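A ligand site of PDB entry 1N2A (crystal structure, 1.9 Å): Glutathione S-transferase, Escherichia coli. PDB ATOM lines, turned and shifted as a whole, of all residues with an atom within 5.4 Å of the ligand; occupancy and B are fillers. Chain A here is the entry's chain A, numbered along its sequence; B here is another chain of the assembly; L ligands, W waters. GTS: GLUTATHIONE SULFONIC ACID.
Water W6 lies within hydrogen-bond range of an oxygen (O11) of the ligand (2.7 Å), the side-chain hydroxyl (OH) of Tyr 157 (2.9 Å), the backbone NH (N) of Val 67 (3.1 Å) and the backbone NH (N) of Gly 66 (3.2 Å). Water W1 lies within hydrogen-bond range of O31 of the ligand (2.8 Å) and NH1 of Arg 114 (3.4 Å). Water W2 lies within hydrogen-bond range of an oxygen (O12) of the ligand (2.8 Å), the backbone carbonyl oxygen of Pro 53 (2.9 Å) and the backbone NH of Glu 65 (2.9 Å). Water W5 bridges O11 of the ligand (2.9 Å) and ND1 of His 106 (3.2 Å). Water W4 bridges O12 of the ligand (3.2 Å) and SG of Cys 10 (3.3 Å). Water W3 bridges the backbone carbonyl oxygen of Lys 49 and an oxygen (O31) of the ligand.
ND1 of His 106 is in hydrogen-bond range of OH of Tyr 157. NZ of Lys 35 lies within hydrogen-bond range of O of Leu 32 (2.8 Å). O of His 106 sits at hydrogen-bond distance from OG1 of Thr 110, at 3.1 Å. The side-chain sulfur of Cys 10 lies within hydrogen-bond range of the backbone carbonyl oxygen of Val 52 (3.3 Å). The side-chain carboxylate of Glu 65 is in hydrogen-bond range of the side-chain amide nitrogen of Asn 99 of chain B, 2.7 Å away. The side-chain carboxylate of Glu 104 of chain B lies within salt-bridge range of the side-chain amino group of Lys 107 (2.7 Å). O of Gly 8 lies within hydrogen-bond range of NE1 of Trp 164. The side-chain carboxylate (OE1) of Glu 104 of chain B lies close to the side-chain amide oxygen (OE1) of Gln 51 (3.1 Å).
CB of Ala 9 touches O2S of the ligand, 3.0 Å away. Leu 32 touches the ligand (CD1 to N3, 3.8 Å). Gln 51 touches the ligand. Pro 53 touches the ligand. Phe 113 touches the ligand. Trp 164 touches the ligand (CZ2 to O2S, 3.4 Å). Hydrophobic or aromatic side chains that line the ligand: Ala 9, Leu 32, Pro 53, His 106, Phe 113 and Trp 164. Of the 25 residues printed, 16 come within 4 Å of the ligand.
An oxygen (O31) of the ligand lies within salt-bridge range of the side-chain amino group of Lys 35, 2.7 Å away. The backbone carbonyl oxygen (O) of Val 52 lies within hydrogen-bond range of a nitrogen (N2) of the ligand, at 3.0 Å. The side-chain hydroxyl (OG1) of Thr 103 of chain B lies within hydrogen-bond range of a nitrogen (N1) of the ligand (2.9 Å). NE2 of His 106 sits at hydrogen-bond distance from O3S of the ligand, 2.5 Å away. O3S of the ligand lies within hydrogen-bond range of SG of Cys 10, 3.4 Å away. The side-chain carboxylate of Glu 65 is in salt-bridge range of a nitrogen (N1) of the ligand (2.6 Å). The side-chain amino group (NZ) of Lys 107 is in hydrogen-bond range of an oxygen (OE1) of the ligand, 3.2 Å away. OE1 of Glu 104 of chain B lies within salt-bridge range of N1 of the ligand (3.0 Å). An oxygen (O2) of the ligand is in hydrogen-bond range of the backbone NH of Val 52 (2.9 Å). The backbone NH of Cys 10 lies within hydrogen-bond range of an oxygen (O2S) of the ligand. The side-chain amide nitrogen (ND2) of Asn 99 of chain B lies within hydrogen-bond range of an oxygen (O11) of the ligand (3.2 Å). An oxygen (O12) of the ligand is in hydrogen-bond range of the backbone NH (N) of Gly 66 (3.0 Å).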
ATOM      1  N   GLY A   8     -22.632  -5.813  10.485  1.00  0.00           N
ATOM      2  CA  GLY A   8     -22.665  -4.622  11.295  1.00  0.00           C
ATOM      3  C   GLY A   8     -21.806  -4.539  12.545  1.00  0.00           C
ATOM      4  O   GLY A   8     -21.726  -3.471  13.177  1.00  0.00           O
ATOM      5  N   ALA A   9     -21.168  -5.651  12.921  1.00  0.00           N
ATOM      6  CA  ALA A   9     -20.181  -5.636  13.987  1.00  0.00           C
ATOM      7  C   ALA A   9     -18.872  -4.885  13.567  1.00  0.00           C
ATOM      8  O   ALA A   9     -18.732  -4.451  12.403  1.00  0.00           O
ATOM      9  CB  ALA A   9     -19.904  -7.087  14.456  1.00  0.00           C
ATOM     10  N   CYS A  10     -17.936  -4.810  14.512  1.00  0.00           N
ATOM     11  CA  CYS A  10     -16.651  -4.100  14.381  1.00  0.00           C
ATOM     12  C   CYS A  10     -15.819  -4.666  13.230  1.00  0.00           C
ATOM     13  O   CYS A  10     -15.067  -3.910  12.608  1.00  0.00           O
ATOM     14  CB  CYS A  10     -15.837  -4.156  15.670  1.00  0.00           C
ATOM     15  SG  CYS A  10     -15.146  -5.822  16.176  1.00  0.00           S
ATOM     16  N   SER A  11     -16.026  -5.941  12.909  1.00  0.00           N
ATOM     17  CA  SER A  11     -15.441  -6.607  11.754  1.00  0.00           C
ATOM     18  C   SER A  11     -15.686  -5.932  10.396  1.00  0.00           C
ATOM     19  O   SER A  11     -14.944  -6.150   9.444  1.00  0.00           O
ATOM     20  CB  SER A  11     -15.944  -8.065  11.680  1.00  0.00           C
ATOM     21  OG  SER A  11     -17.373  -8.131  11.833  1.00  0.00           O
ATOM     22  N   LEU A  32     -22.636 -14.905  17.276  1.00  0.00           N
ATOM     23  CA  LEU A  32     -21.840 -14.580  18.468  1.00  0.00           C
ATOM     24  C   LEU A  32     -22.476 -15.052  19.764  1.00  0.00           C
ATOM     25  O   LEU A  32     -21.787 -15.273  20.739  1.00  0.00           O
ATOM     26  CB  LEU A  32     -21.574 -13.081  18.536  1.00  0.00           C
ATOM     27  CG  LEU A  32     -20.754 -12.554  17.347  1.00  0.00           C
ATOM     28  CD1 LEU A  32     -20.549 -11.098  17.578  1.00  0.00           C
ATOM     29  CD2 LEU A  32     -19.427 -13.267  17.226  1.00  0.00           C
ATOM     30  N   LYS A  35     -21.631 -18.803  19.515  1.00  0.00           N
ATOM     31  CA  LYS A  35     -20.268 -19.047  19.031  1.00  0.00           C
ATOM     32  C   LYS A  35     -20.223 -20.177  18.002  1.00  0.00           C
ATOM     33  O   LYS A  35     -19.365 -21.078  18.041  1.00  0.00           O
ATOM     34  CB  LYS A  35     -19.326 -19.319  20.213  1.00  0.00           C
ATOM     35  CG  LYS A  35     -18.664 -18.066  20.742  1.00  0.00           C
ATOM     36  CD  LYS A  35     -19.560 -17.295  21.729  1.00  0.00           C
ATOM     37  CE  LYS A  35     -18.828 -16.078  22.315  1.00  0.00           C
ATOM     38  NZ  LYS A  35     -19.134 -14.818  21.579  1.00  0.00           N
ATOM     39  N   LYS A  49     -10.466 -16.782  21.323  1.00  0.00           N
ATOM     40  CA  LYS A  49     -11.019 -15.640  22.036  1.00  0.00           C
ATOM     41  C   LYS A  49     -12.560 -15.497  21.766  1.00  0.00           C
ATOM     42  O   LYS A  49     -13.233 -14.741  22.452  1.00  0.00           O
ATOM     43  CB  LYS A  49     -10.219 -14.345  21.736  1.00  0.00           C
ATOM     44  CG  LYS A  49      -8.710 -14.461  22.065  1.00  0.00           C
ATOM     45  CD  LYS A  49      -7.784 -13.186  21.771  1.00  0.00           C
ATOM     46  CE  LYS A  49      -7.373 -13.064  20.326  1.00  0.00           C
ATOM     47  NZ  LYS A  49      -6.405 -11.908  20.151  1.00  0.00           N
ATOM     48  N   GLY A  50     -13.063 -16.215  20.766  1.00  0.00           N
ATOM     49  CA  GLY A  50     -14.455 -16.261  20.384  1.00  0.00           C
ATOM     50  C   GLY A  50     -15.037 -14.962  19.856  1.00  0.00           C
ATOM     51  O   GLY A  50     -16.225 -14.774  19.931  1.00  0.00           O
ATOM     52  N   GLN A  51     -14.211 -14.051  19.337  1.00  0.00           N
ATOM     53  CA  GLN A  51     -14.699 -12.734  18.884  1.00  0.00           C
ATOM     54  C   GLN A  51     -14.513 -12.591  17.393  1.00  0.00           C
ATOM     55  O   GLN A  51     -13.710 -13.292  16.819  1.00  0.00           O
ATOM     56  CB  GLN A  51     -13.882 -11.673  19.500  1.00  0.00           C
ATOM     57  CG  GLN A  51     -13.991 -11.544  20.989  1.00  0.00           C
ATOM     58  CD  GLN A  51     -12.972 -10.569  21.491  1.00  0.00           C
ATOM     59  OE1 GLN A  51     -13.217  -9.825  22.412  1.00  0.00           O
ATOM     60  NE2 GLN A  51     -11.800 -10.564  20.846  1.00  0.00           N
ATOM     61  N   VAL A  52     -15.279 -11.692  16.765  1.00  0.00           N
ATOM     62  CA  VAL A  52     -14.948 -11.244  15.390  1.00  0.00           C
ATOM     63  C   VAL A  52     -14.293  -9.820  15.455  1.00  0.00           C
ATOM     64  O   VAL A  52     -14.565  -9.019  16.385  1.00  0.00           O
ATOM     65  CB  VAL A  52     -16.182 -11.300  14.444  1.00  0.00           C
ATOM     66  CG1 VAL A  52     -16.715 -12.717  14.322  1.00  0.00           C
ATOM     67  CG2 VAL A  52     -17.296 -10.401  14.887  1.00  0.00           C
ATOM     68  N   PRO A  53     -13.441  -9.470  14.490  1.00  0.00           N
ATOM     69  CA  PRO A  53     -13.109 -10.243  13.297  1.00  0.00           C
ATOM     70  C   PRO A  53     -12.024 -11.265  13.573  1.00  0.00           C
ATOM     71  O   PRO A  53     -11.337 -11.210  14.554  1.00  0.00           O
ATOM     72  CB  PRO A  53     -12.464  -9.201  12.390  1.00  0.00           C
ATOM     73  CG  PRO A  53     -11.787  -8.269  13.378  1.00  0.00           C
ATOM     74  CD  PRO A  53     -12.718  -8.190  14.519  1.00  0.00           C
ATOM     75  N   GLU A  65      -7.798  -9.417  16.180  1.00  0.00           N
ATOM     76  CA  GLU A  65      -7.720  -8.008  16.582  1.00  0.00           C
ATOM     77  C   GLU A  65      -7.819  -7.098  15.382  1.00  0.00           C
ATOM     78  O   GLU A  65      -6.877  -7.034  14.565  1.00  0.00           O
ATOM     79  CB  GLU A  65      -6.482  -7.659  17.443  1.00  0.00           C
ATOM     80  CG  GLU A  65      -6.330  -8.489  18.709  1.00  0.00           C
ATOM     81  CD  GLU A  65      -7.381  -8.230  19.759  1.00  0.00           C
ATOM     82  OE1 GLU A  65      -7.903  -7.101  19.898  1.00  0.00           O
ATOM     83  OE2 GLU A  65      -7.673  -9.236  20.417  1.00  0.00           O
ATOM     84  N   GLY A  66      -8.919  -6.348  15.260  1.00  0.00           N
ATOM     85  CA  GLY A  66      -9.196  -5.610  14.006  1.00  0.00           C
ATOM     86  C   GLY A  66      -8.054  -4.682  13.597  1.00  0.00           C
ATOM     87  O   GLY A  66      -7.631  -4.599  12.433  1.00  0.00           O
ATOM     88  N   VAL A  67      -7.528  -3.959  14.572  1.00  0.00           N
ATOM     89  CA  VAL A  67      -6.393  -3.050  14.327  1.00  0.00           C
ATOM     90  C   VAL A  67      -5.161  -3.775  13.711  1.00  0.00           C
ATOM     91  O   VAL A  67      -4.472  -3.218  12.808  1.00  0.00           O
ATOM     92  CB  VAL A  67      -6.009  -2.333  15.636  1.00  0.00           C
ATOM     93  CG1 VAL A  67      -4.655  -1.682  15.556  1.00  0.00           C
ATOM     94  CG2 VAL A  67      -7.069  -1.237  16.011  1.00  0.00           C
ATOM     95  N   HIS A 106     -15.074   2.030  20.321  1.00  0.00           N
ATOM     96  CA  HIS A 106     -15.429   0.611  20.189  1.00  0.00           C
ATOM     97  C   HIS A 106     -15.703  -0.052  21.531  1.00  0.00           C
ATOM     98  O   HIS A 106     -16.773  -0.612  21.732  1.00  0.00           O
ATOM     99  CB  HIS A 106     -14.277  -0.102  19.531  1.00  0.00           C
ATOM    100  CG  HIS A 106     -14.520  -1.563  19.218  1.00  0.00           C
ATOM    101  ND1 HIS A 106     -13.631  -2.270  18.451  1.00  0.00           N
ATOM    102  CD2 HIS A 106     -15.487  -2.449  19.612  1.00  0.00           C
ATOM    103  CE1 HIS A 106     -14.064  -3.524  18.321  1.00  0.00           C
ATOM    104  NE2 HIS A 106     -15.199  -3.654  19.011  1.00  0.00           N
ATOM    105  N   LYS A 107     -14.743   0.019  22.472  1.00  0.00           N
ATOM    106  CA  LYS A 107     -14.967  -0.602  23.775  1.00  0.00           C
ATOM    107  C   LYS A 107     -15.845   0.282  24.674  1.00  0.00           C
ATOM    108  O   LYS A 107     -16.398  -0.190  25.668  1.00  0.00           O
ATOM    109  CB  LYS A 107     -13.646  -0.967  24.475  1.00  0.00           C
ATOM    110  CG  LYS A 107     -13.002  -2.278  23.984  1.00  0.00           C
ATOM    111  CD  LYS A 107     -13.943  -3.504  24.080  1.00  0.00           C
ATOM    112  CE  LYS A 107     -13.398  -4.702  23.323  1.00  0.00           C
ATOM    113  NZ  LYS A 107     -14.039  -6.035  23.577  1.00  0.00           N
ATOM    114  N   THR A 110     -19.362  -1.266  23.703  1.00  0.00           N
ATOM    115  CA  THR A 110     -19.500  -2.688  24.004  1.00  0.00           C
ATOM    116  C   THR A 110     -20.481  -3.020  25.111  1.00  0.00           C
ATOM    117  O   THR A 110     -21.307  -3.937  24.963  1.00  0.00           O
ATOM    118  CB  THR A 110     -18.106  -3.322  24.365  1.00  0.00           C
ATOM    119  OG1 THR A 110     -17.264  -3.250  23.250  1.00  0.00           O
ATOM    120  CG2 THR A 110     -18.245  -4.838  24.599  1.00  0.00           C
ATOM    121  N   PHE A 113     -23.933  -3.606  24.219  1.00  0.00           N
ATOM    122  CA  PHE A 113     -24.265  -4.805  23.441  1.00  0.00           C
ATOM    123  C   PHE A 113     -24.244  -6.109  24.244  1.00  0.00           C
ATOM    124  O   PHE A 113     -24.524  -7.170  23.686  1.00  0.00           O
ATOM    125  CB  PHE A 113     -23.298  -4.966  22.235  1.00  0.00           C
ATOM    126  CG  PHE A 113     -23.177  -3.734  21.369  1.00  0.00           C
ATOM    127  CD1 PHE A 113     -24.221  -2.831  21.286  1.00  0.00           C
ATOM    128  CD2 PHE A 113     -22.018  -3.480  20.654  1.00  0.00           C
ATOM    129  CE1 PHE A 113     -24.141  -1.708  20.511  1.00  0.00           C
ATOM    130  CE2 PHE A 113     -21.936  -2.332  19.841  1.00  0.00           C
ATOM    131  CZ  PHE A 113     -23.016  -1.452  19.791  1.00  0.00           C
ATOM    132  N   ARG A 114     -23.893  -6.069  25.526  1.00  0.00           N
ATOM    133  CA  ARG A 114     -23.714  -7.297  26.296  1.00  0.00           C
ATOM    134  C   ARG A 114     -24.924  -7.568  27.190  1.00  0.00           C
ATOM    135  O   ARG A 114     -25.554  -6.633  27.668  1.00  0.00           O
ATOM    136  CB  ARG A 114     -22.464  -7.198  27.167  1.00  0.00           C
ATOM    137  CG  ARG A 114     -21.152  -7.337  26.410  1.00  0.00           C
ATOM    138  CD  ARG A 114     -19.947  -7.169  27.296  1.00  0.00           C
ATOM    139  NE  ARG A 114     -19.807  -8.330  28.178  1.00  0.00           N
ATOM    140  CZ  ARG A 114     -19.053  -9.403  27.912  1.00  0.00           C
ATOM    141  NH1 ARG A 114     -18.307  -9.445  26.803  1.00  0.00           N
ATOM    142  NH2 ARG A 114     -19.023 -10.419  28.771  1.00  0.00           N
ATOM    143  N   TYR A 157     -12.350   2.416  10.259  1.00  0.00           N
ATOM    144  CA  TYR A 157     -12.689   1.982  11.651  1.00  0.00           C
ATOM    145  C   TYR A 157     -13.634   2.950  12.298  1.00  0.00           C
ATOM    146  O   TYR A 157     -14.600   2.553  12.928  1.00  0.00           O
ATOM    147  CB  TYR A 157     -11.412   1.814  12.478  1.00  0.00           C
ATOM    148  CG  TYR A 157     -11.435   0.990  13.800  1.00  0.00           C
ATOM    149  CD1 TYR A 157     -12.516   0.210  14.183  1.00  0.00           C
ATOM    150  CD2 TYR A 157     -10.360   1.071  14.692  1.00  0.00           C
ATOM    151  CE1 TYR A 157     -12.472  -0.564  15.346  1.00  0.00           C
ATOM    152  CE2 TYR A 157     -10.337   0.362  15.866  1.00  0.00           C
ATOM    153  CZ  TYR A 157     -11.401  -0.489  16.191  1.00  0.00           C
ATOM    154  OH  TYR A 157     -11.391  -1.226  17.363  1.00  0.00           O
ATOM    155  N   TRP A 164     -22.792   2.864  15.041  1.00  0.00           N
ATOM    156  CA  TRP A 164     -23.465   2.435  16.266  1.00  0.00           C
ATOM    157  C   TRP A 164     -24.156   3.560  17.022  1.00  0.00           C
ATOM    158  O   TRP A 164     -25.127   3.320  17.806  1.00  0.00           O
ATOM    159  CB  TRP A 164     -22.522   1.699  17.175  1.00  0.00           C
ATOM    160  CG  TRP A 164     -21.969   0.432  16.617  1.00  0.00           C
ATOM    161  CD1 TRP A 164     -22.508  -0.355  15.594  1.00  0.00           C
ATOM    162  CD2 TRP A 164     -20.796  -0.220  17.058  1.00  0.00           C
ATOM    163  NE1 TRP A 164     -21.741  -1.480  15.437  1.00  0.00           N
ATOM    164  CE2 TRP A 164     -20.653  -1.406  16.285  1.00  0.00           C
ATOM    165  CE3 TRP A 164     -19.821   0.080  18.027  1.00  0.00           C
ATOM    166  CZ2 TRP A 164     -19.615  -2.292  16.474  1.00  0.00           C
ATOM    167  CZ3 TRP A 164     -18.774  -0.819  18.229  1.00  0.00           C
ATOM    168  CH2 TRP A 164     -18.680  -1.988  17.443  1.00  0.00           C
ATOM    169  N   ASN B  99      -3.016  -4.614  20.898  1.00  0.00           N
ATOM    170  CA  ASN B  99      -4.440  -4.259  20.841  1.00  0.00           C
ATOM    171  C   ASN B  99      -5.224  -5.052  21.892  1.00  0.00           C
ATOM    172  O   ASN B  99      -6.097  -4.498  22.543  1.00  0.00           O
ATOM    173  CB  ASN B  99      -5.038  -4.492  19.458  1.00  0.00           C
ATOM    174  CG  ASN B  99      -6.350  -3.774  19.295  1.00  0.00           C
ATOM    175  OD1 ASN B  99      -6.402  -2.536  19.306  1.00  0.00           O
ATOM    176  ND2 ASN B  99      -7.412  -4.533  19.243  1.00  0.00           N
ATOM    177  N   TYR B 100      -4.907  -6.327  22.064  1.00  0.00           N
ATOM    178  CA  TYR B 100      -5.578  -7.161  23.067  1.00  0.00           C
ATOM    179  C   TYR B 100      -5.387  -6.564  24.422  1.00  0.00           C
ATOM    180  O   TYR B 100      -6.340  -6.435  25.238  1.00  0.00           O
ATOM    181  CB  TYR B 100      -5.024  -8.582  23.006  1.00  0.00           C
ATOM    182  CG  TYR B 100      -5.624  -9.518  24.065  1.00  0.00           C
ATOM    183  CD1 TYR B 100      -4.998  -9.668  25.288  1.00  0.00           C
ATOM    184  CD2 TYR B 100      -6.793 -10.177  23.831  1.00  0.00           C
ATOM    185  CE1 TYR B 100      -5.512 -10.506  26.262  1.00  0.00           C
ATOM    186  CE2 TYR B 100      -7.343 -11.026  24.802  1.00  0.00           C
ATOM    187  CZ  TYR B 100      -6.673 -11.188  26.002  1.00  0.00           C
ATOM    188  OH  TYR B 100      -7.195 -12.026  26.922  1.00  0.00           O
ATOM    189  N   THR B 103      -7.402  -3.134  24.761  1.00  0.00           N
ATOM    190  CA  THR B 103      -8.859  -3.135  24.666  1.00  0.00           C
ATOM    191  C   THR B 103      -9.452  -4.144  25.657  1.00  0.00           C
ATOM    192  O   THR B 103     -10.546  -3.922  26.173  1.00  0.00           O
ATOM    193  CB  THR B 103      -9.384  -3.469  23.265  1.00  0.00           C
ATOM    194  OG1 THR B 103      -8.891  -4.732  22.778  1.00  0.00           O
ATOM    195  CG2 THR B 103      -8.947  -2.443  22.196  1.00  0.00           C
ATOM    196  N   GLU B 104      -8.736  -5.225  25.967  1.00  0.00           N
ATOM    197  CA  GLU B 104      -9.304  -6.308  26.760  1.00  0.00           C
ATOM    198  C   GLU B 104      -8.770  -6.285  28.163  1.00  0.00           C
ATOM    199  O   GLU B 104      -9.458  -6.691  29.050  1.00  0.00           O
ATOM    200  CB  GLU B 104      -9.086  -7.685  26.127  1.00  0.00           C
ATOM    201  CG  GLU B 104      -9.637  -7.868  24.728  1.00  0.00           C
ATOM    202  CD  GLU B 104     -11.151  -7.688  24.620  1.00  0.00           C
ATOM    203  OE1 GLU B 104     -11.631  -7.361  23.533  1.00  0.00           O
ATOM    204  OE2 GLU B 104     -11.868  -7.876  25.613  1.00  0.00           O
HETATM  205  N1  GTS L   1     -10.243  -6.611  20.976  1.00  0.00           N
HETATM  206  CA1 GTS L   1     -11.110  -7.154  19.874  1.00  0.00           C
HETATM  207  C1  GTS L   1     -10.536  -6.530  18.617  1.00  0.00           C
HETATM  208  O11 GTS L   1     -10.487  -5.126  18.680  1.00  0.00           O
HETATM  209  O12 GTS L   1     -10.946  -6.980  17.352  1.00  0.00           O
HETATM  210  CB1 GTS L   1     -12.611  -6.872  20.156  1.00  0.00           C
HETATM  211  CG1 GTS L   1     -13.520  -7.480  19.067  1.00  0.00           C
HETATM  212  CD1 GTS L   1     -15.019  -7.252  19.417  1.00  0.00           C
HETATM  213  OE1 GTS L   1     -15.239  -6.956  20.768  1.00  0.00           O
HETATM  214  N2  GTS L   1     -15.889  -8.277  18.954  1.00  0.00           N
HETATM  215  CA2 GTS L   1     -17.296  -8.333  19.380  1.00  0.00           C
HETATM  216  C2  GTS L   1     -17.324  -9.750  19.924  1.00  0.00           C
HETATM  217  O2  GTS L   1     -16.974 -10.659  18.910  1.00  0.00           O
HETATM  218  CB2 GTS L   1     -18.182  -7.884  18.244  1.00  0.00           C
HETATM  219  SG2 GTS L   1     -18.444  -6.061  18.354  1.00  0.00           S
HETATM  220  O1S GTS L   1     -19.457  -5.855  19.672  1.00  0.00           O
HETATM  221  O2S GTS L   1     -19.369  -5.630  17.036  1.00  0.00           O
HETATM  222  O3S GTS L   1     -17.128  -5.211  18.927  1.00  0.00           O
HETATM  223  N3  GTS L   1     -18.478 -10.157  20.648  1.00  0.00           N
HETATM  224  CA3 GTS L   1     -18.554 -11.521  21.152  1.00  0.00           C
HETATM  225  C3  GTS L   1     -17.590 -11.836  22.298  1.00  0.00           C
HETATM  226  O31 GTS L   1     -18.268 -12.771  23.098  1.00  0.00           O
HETATM  227  O32 GTS L   1     -17.188 -10.706  23.117  1.00  0.00           O
HETATM  228  O   HOH W   1     -18.255 -12.749  25.886  1.00  0.00           O
HETATM  229  O   HOH W   2     -10.592  -9.738  16.912  1.00  0.00           O
HETATM  230  O   HOH W   3     -15.844 -14.846  23.493  1.00  0.00           O
HETATM  231  O   HOH W   4     -12.117  -4.771  15.374  1.00  0.00           O
HETATM  232  O   HOH W   5     -11.612  -3.312  20.707  1.00  0.00           O
HETATM  233  O   HOH W   6      -9.823  -3.563  16.555  1.00  0.00           O
